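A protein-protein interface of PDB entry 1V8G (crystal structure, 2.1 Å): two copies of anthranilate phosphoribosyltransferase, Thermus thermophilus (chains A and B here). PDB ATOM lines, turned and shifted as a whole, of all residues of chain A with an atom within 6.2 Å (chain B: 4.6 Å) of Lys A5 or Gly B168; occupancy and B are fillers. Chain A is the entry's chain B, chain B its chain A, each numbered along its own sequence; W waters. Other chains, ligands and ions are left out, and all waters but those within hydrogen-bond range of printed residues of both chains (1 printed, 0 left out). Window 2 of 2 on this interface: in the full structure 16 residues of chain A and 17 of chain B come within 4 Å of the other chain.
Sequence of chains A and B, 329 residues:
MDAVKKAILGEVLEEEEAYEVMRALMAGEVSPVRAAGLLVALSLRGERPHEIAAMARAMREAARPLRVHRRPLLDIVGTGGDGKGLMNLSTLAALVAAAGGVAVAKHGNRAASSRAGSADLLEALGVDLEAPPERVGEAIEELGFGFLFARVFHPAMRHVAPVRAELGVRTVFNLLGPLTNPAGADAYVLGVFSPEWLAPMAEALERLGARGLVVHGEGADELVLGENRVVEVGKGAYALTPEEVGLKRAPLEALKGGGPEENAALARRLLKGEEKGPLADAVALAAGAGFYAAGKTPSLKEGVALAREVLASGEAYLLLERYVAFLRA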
ATOM      1  N   MET A   1     -20.862  22.701 -11.300  1.00  0.00           N
ATOM      2  CA  MET A   1     -19.562  22.249 -10.730  1.00  0.00           C
ATOM      3  C   MET A   1     -19.089  23.163  -9.607  1.00  0.00           C
ATOM      4  O   MET A   1     -19.328  24.372  -9.629  1.00  0.00           O
ATOM      5  CB  MET A   1     -18.493  22.196 -11.826  1.00  0.00           C
ATOM      6  CG  MET A   1     -17.074  21.974 -11.306  1.00  0.00           C
ATOM      7  SD  MET A   1     -15.847  21.762 -12.615  1.00  0.00           S
ATOM      8  CE  MET A   1     -15.668  23.452 -13.215  1.00  0.00           C
ATOM      9  N   ASP A   2     -18.414  22.569  -8.626  1.00  0.00           N
ATOM     10  CA  ASP A   2     -17.883  23.308  -7.489  1.00  0.00           C
ATOM     11  C   ASP A   2     -17.080  24.510  -7.977  1.00  0.00           C
ATOM     12  O   ASP A   2     -16.326  24.407  -8.943  1.00  0.00           O
ATOM     13  CB  ASP A   2     -16.989  22.393  -6.649  1.00  0.00           C
ATOM     14  CG  ASP A   2     -16.270  23.137  -5.546  1.00  0.00           C
ATOM     15  OD1 ASP A   2     -16.939  23.591  -4.592  1.00  0.00           O
ATOM     16  OD2 ASP A   2     -15.032  23.276  -5.643  1.00  0.00           O
ATOM     17  N   ALA A   3     -17.242  25.646  -7.305  1.00  0.00           N
ATOM     18  CA  ALA A   3     -16.543  26.870  -7.686  1.00  0.00           C
ATOM     19  C   ALA A   3     -15.034  26.802  -7.448  1.00  0.00           C
ATOM     20  O   ALA A   3     -14.259  27.414  -8.185  1.00  0.00           O
ATOM     21  CB  ALA A   3     -17.132  28.061  -6.933  1.00  0.00           C
ATOM     22  N   VAL A   4     -14.623  26.069  -6.416  1.00  0.00           N
ATOM     23  CA  VAL A   4     -13.206  25.935  -6.091  1.00  0.00           C
ATOM     24  C   VAL A   4     -12.523  25.032  -7.110  1.00  0.00           C
ATOM     25  O   VAL A   4     -11.393  25.291  -7.523  1.00  0.00           O
ATOM     26  CB  VAL A   4     -13.005  25.338  -4.676  1.00  0.00           C
ATOM     27  CG1 VAL A   4     -11.503  25.179  -4.380  1.00  0.00           C
ATOM     28  CG2 VAL A   4     -13.662  26.242  -3.635  1.00  0.00           C
ATOM     29  N   LYS A   5     -13.214  23.972  -7.515  1.00  0.00           N
ATOM     30  CA  LYS A   5     -12.656  23.054  -8.498  1.00  0.00           C
ATOM     31  C   LYS A   5     -12.521  23.772  -9.831  1.00  0.00           C
ATOM     32  O   LYS A   5     -11.548  23.569 -10.561  1.00  0.00           O
ATOM     33  CB  LYS A   5     -13.543  21.819  -8.660  1.00  0.00           C
ATOM     34  CG  LYS A   5     -13.034  20.847  -9.711  1.00  0.00           C
ATOM     35  CD  LYS A   5     -13.784  19.525  -9.659  1.00  0.00           C
ATOM     36  CE  LYS A   5     -13.342  18.605 -10.781  1.00  0.00           C
ATOM     37  NZ  LYS A   5     -13.898  17.244 -10.612  1.00  0.00           N
ATOM     38  N   LYS A   6     -13.495  24.622 -10.138  1.00  0.00           N
ATOM     39  CA  LYS A   6     -13.470  25.373 -11.381  1.00  0.00           C
ATOM     40  C   LYS A   6     -12.277  26.316 -11.384  1.00  0.00           C
ATOM     41  O   LYS A   6     -11.616  26.495 -12.407  1.00  0.00           O
ATOM     42  CB  LYS A   6     -14.762  26.177 -11.557  1.00  0.00           C
ATOM     43  CG  LYS A   6     -14.789  26.974 -12.848  1.00  0.00           C
ATOM     44  CD  LYS A   6     -16.092  27.733 -13.032  1.00  0.00           C
ATOM     45  CE  LYS A   6     -16.073  28.511 -14.342  1.00  0.00           C
ATOM     46  NZ  LYS A   6     -17.311  29.314 -14.540  1.00  0.00           N
ATOM     47  N   ALA A   7     -12.005  26.930 -10.240  1.00  0.00           N
ATOM     48  CA  ALA A   7     -10.873  27.843 -10.140  1.00  0.00           C
ATOM     49  C   ALA A   7      -9.571  27.060 -10.313  1.00  0.00           C
ATOM     50  O   ALA A   7      -8.674  27.479 -11.046  1.00  0.00           O
ATOM     51  CB  ALA A   7     -10.886  28.548  -8.791  1.00  0.00           C
ATOM     52  N   ILE A   8      -9.483  25.918  -9.642  1.00  0.00           N
ATOM     53  CA  ILE A   8      -8.294  25.073  -9.713  1.00  0.00           C
ATOM     54  C   ILE A   8      -8.047  24.627 -11.152  1.00  0.00           C
ATOM     55  O   ILE A   8      -6.900  24.436 -11.563  1.00  0.00           O
ATOM     56  CB  ILE A   8      -8.435  23.833  -8.794  1.00  0.00           C
ATOM     57  CG1 ILE A   8      -8.469  24.284  -7.330  1.00  0.00           C
ATOM     58  CG2 ILE A   8      -7.284  22.848  -9.042  1.00  0.00           C
ATOM     59  CD1 ILE A   8      -8.728  23.165  -6.326  1.00  0.00           C
ATOM     60  N   LEU A   9      -9.128  24.472 -11.911  1.00  0.00           N
ATOM     61  CA  LEU A   9      -9.036  24.069 -13.311  1.00  0.00           C
ATOM     62  C   LEU A   9      -8.591  25.238 -14.183  1.00  0.00           C
ATOM     63  O   LEU A   9      -8.427  25.097 -15.392  1.00  0.00           O
ATOM     64  CB  LEU A   9     -10.380  23.522 -13.797  1.00  0.00           C
ATOM     65  CG  LEU A   9     -10.714  22.144 -13.226  1.00  0.00           C
ATOM     66  CD1 LEU A   9     -12.145  21.749 -13.560  1.00  0.00           C
ATOM     67  CD2 LEU A   9      -9.733  21.134 -13.798  1.00  0.00           C
ATOM     68  N   GLY A  10      -8.403  26.397 -13.561  1.00  0.00           N
ATOM     69  CA  GLY A  10      -7.940  27.564 -14.288  1.00  0.00           C
ATOM     70  C   GLY A  10      -8.973  28.297 -15.119  1.00  0.00           C
ATOM     71  O   GLY A  10      -8.620  29.175 -15.902  1.00  0.00           O
ATOM     72  N   GLU A  11     -10.243  27.942 -14.961  1.00  0.00           N
ATOM     73  CA  GLU A  11     -11.310  28.595 -15.704  1.00  0.00           C
ATOM     74  C   GLU A  11     -11.620  29.949 -15.079  1.00  0.00           C
ATOM     75  O   GLU A  11     -11.495  30.123 -13.864  1.00  0.00           O
ATOM     76  CB  GLU A  11     -12.569  27.722 -15.708  1.00  0.00           C
ATOM     77  CG  GLU A  11     -12.437  26.445 -16.532  1.00  0.00           C
ATOM     78  CD  GLU A  11     -13.699  25.593 -16.503  1.00  0.00           C
ATOM     79  OE1 GLU A  11     -14.800  26.156 -16.680  1.00  0.00           O
ATOM     80  OE2 GLU A  11     -13.592  24.361 -16.313  1.00  0.00           O
ATOM     81  N   ARG A  34      -6.454  22.668  -1.318  1.00  0.00           N
ATOM     82  CA  ARG A  34      -7.285  23.331  -2.313  1.00  0.00           C
ATOM     83  C   ARG A  34      -7.138  24.845  -2.273  1.00  0.00           C
ATOM     84  O   ARG A  34      -7.264  25.510  -3.298  1.00  0.00           O
ATOM     85  CB  ARG A  34      -8.750  22.916  -2.132  1.00  0.00           C
ATOM     86  CG  ARG A  34      -8.940  21.406  -2.248  1.00  0.00           C
ATOM     87  CD  ARG A  34     -10.393  20.996  -2.090  1.00  0.00           C
ATOM     88  NE  ARG A  34     -11.162  21.240  -3.302  1.00  0.00           N
ATOM     89  CZ  ARG A  34     -12.416  21.675  -3.312  1.00  0.00           C
ATOM     90  NH1 ARG A  34     -13.043  21.923  -2.168  1.00  0.00           N
ATOM     91  NH2 ARG A  34     -13.048  21.846  -4.466  1.00  0.00           N
ATOM     92  N   ARG B 164      -3.123  14.423  -4.425  1.00  0.00           N
ATOM     93  CA  ARG B 164      -3.770  14.186  -5.717  1.00  0.00           C
ATOM     94  C   ARG B 164      -5.280  14.022  -5.556  1.00  0.00           C
ATOM     95  O   ARG B 164      -6.065  14.598  -6.315  1.00  0.00           O
ATOM     96  CB  ARG B 164      -3.207  12.922  -6.377  1.00  0.00           C
ATOM     97  CG  ARG B 164      -1.736  12.989  -6.754  1.00  0.00           C
ATOM     98  CD  ARG B 164      -1.290  11.660  -7.359  1.00  0.00           C
ATOM     99  NE  ARG B 164      -2.058  11.321  -8.554  1.00  0.00           N
ATOM    100  CZ  ARG B 164      -1.951  10.173  -9.220  1.00  0.00           C
ATOM    101  NH1 ARG B 164      -1.105   9.235  -8.809  1.00  0.00           N
ATOM    102  NH2 ARG B 164      -2.684   9.966 -10.306  1.00  0.00           N
ATOM    103  N   ALA B 165      -5.677  13.227  -4.566  1.00  0.00           N
ATOM    104  CA  ALA B 165      -7.087  12.975  -4.299  1.00  0.00           C
ATOM    105  C   ALA B 165      -7.805  14.242  -3.858  1.00  0.00           C
ATOM    106  O   ALA B 165      -8.949  14.489  -4.247  1.00  0.00           O
ATOM    107  CB  ALA B 165      -7.231  11.899  -3.225  1.00  0.00           C
ATOM    108  N   GLU B 166      -7.122  15.044  -3.046  1.00  0.00           N
ATOM    109  CA  GLU B 166      -7.693  16.275  -2.530  1.00  0.00           C
ATOM    110  C   GLU B 166      -7.881  17.364  -3.592  1.00  0.00           C
ATOM    111  O   GLU B 166      -8.886  18.073  -3.576  1.00  0.00           O
ATOM    112  CB  GLU B 166      -6.831  16.804  -1.381  1.00  0.00           C
ATOM    113  CG  GLU B 166      -7.387  18.057  -0.729  1.00  0.00           C
ATOM    114  CD  GLU B 166      -8.756  17.838  -0.097  1.00  0.00           C
ATOM    115  OE1 GLU B 166      -9.280  16.705  -0.157  1.00  0.00           O
ATOM    116  OE2 GLU B 166      -9.308  18.804   0.463  1.00  0.00           O
ATOM    117  N   LEU B 167      -6.917  17.506  -4.502  1.00  0.00           N
ATOM    118  CA  LEU B 167      -7.008  18.505  -5.573  1.00  0.00           C
ATOM    119  C   LEU B 167      -8.199  18.238  -6.483  1.00  0.00           C
ATOM    120  O   LEU B 167      -8.808  19.175  -7.013  1.00  0.00           O
ATOM    121  CB  LEU B 167      -5.736  18.512  -6.422  1.00  0.00           C
ATOM    122  CG  LEU B 167      -4.526  19.265  -5.877  1.00  0.00           C
ATOM    123  CD1 LEU B 167      -3.350  19.023  -6.798  1.00  0.00           C
ATOM    124  CD2 LEU B 167      -4.837  20.762  -5.778  1.00  0.00           C
ATOM    125  N   GLY B 168      -8.498  16.954  -6.680  1.00  0.00           N
ATOM    126  CA  GLY B 168      -9.621  16.544  -7.504  1.00  0.00           C
ATOM    127  C   GLY B 168      -9.485  16.702  -9.008  1.00  0.00           C
ATOM    128  O   GLY B 168     -10.489  16.677  -9.721  1.00  0.00           O
ATOM    129  N   VAL B 169      -8.262  16.864  -9.502  1.00  0.00           N
ATOM    130  CA  VAL B 169      -8.049  17.025 -10.937  1.00  0.00           C
ATOM    131  C   VAL B 169      -6.805  16.271 -11.390  1.00  0.00           C
ATOM    132  O   VAL B 169      -6.032  15.769 -10.568  1.00  0.00           O
ATOM    133  CB  VAL B 169      -7.884  18.520 -11.326  1.00  0.00           C
ATOM    134  CG1 VAL B 169      -9.051  19.330 -10.785  1.00  0.00           C
ATOM    135  CG2 VAL B 169      -6.562  19.063 -10.794  1.00  0.00           C
HETATM  136  O   HOH W   1     -11.021  20.289  -6.183  1.00  0.00           O
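Met A1 touches none of the printed residues of chain B. Asp A2 touches none of the printed residues of chain B. Lys A5 touches just one residue of chain B: Gly B168. Of the printed residues of chain B, Leu A9 touches Val B169 (3.6 Å). Of the printed residues of chain A, Glu B166 touches Arg A34 (3.5 Å). Gly B168 touches just one residue of chain A: Lys A5 (3.6 Å). The nearest printed residue of chain B that does not touch Arg A34 is Leu B167 (4.8 Å).
No position is printed for both chains. Of the 3 pairs that touch across the chains among the printed residues, none has its exchanged pair printed and touching as well.
Among the printed residues, pairs that only touch across the chains: Arg A34 with Glu B166, Lys A5 with Gly B168 and Leu A9 with Val B169.
Of the 12 printed residues of chain A, 3 touch a printed residue of chain B. Hydrophobic or aromatic side chains of chain A within 4 Å of the printed part of chain B: Leu A9. Of the 6 printed residues of chain B, 3 touch a printed residue of chain A. Hydrophobic or aromatic side chains of chain B within 4 Å of the printed part of chain A: Val B169. Among the printed residues, 3 pairs touch across the chains. Among the printed residues, no Asp or Glu carboxylate lies within 4 Å of a Lys or Arg side-chain nitrogen of the other chain.
The side-chain carboxylate (OD2) of Asp A2 lies within hydrogen-bond range of the backbone NH (N) of Lys A5, at 2.7 Å. NH2 of Arg A34 lies within salt-bridge range of OD2 of Asp A2 (2.7 Å).
Water W1 lies within hydrogen-bond range of the backbone carbonyl oxygen of Leu B167 (2.6 Å) and the guanidinium group of Arg A34 (3.0 Å).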
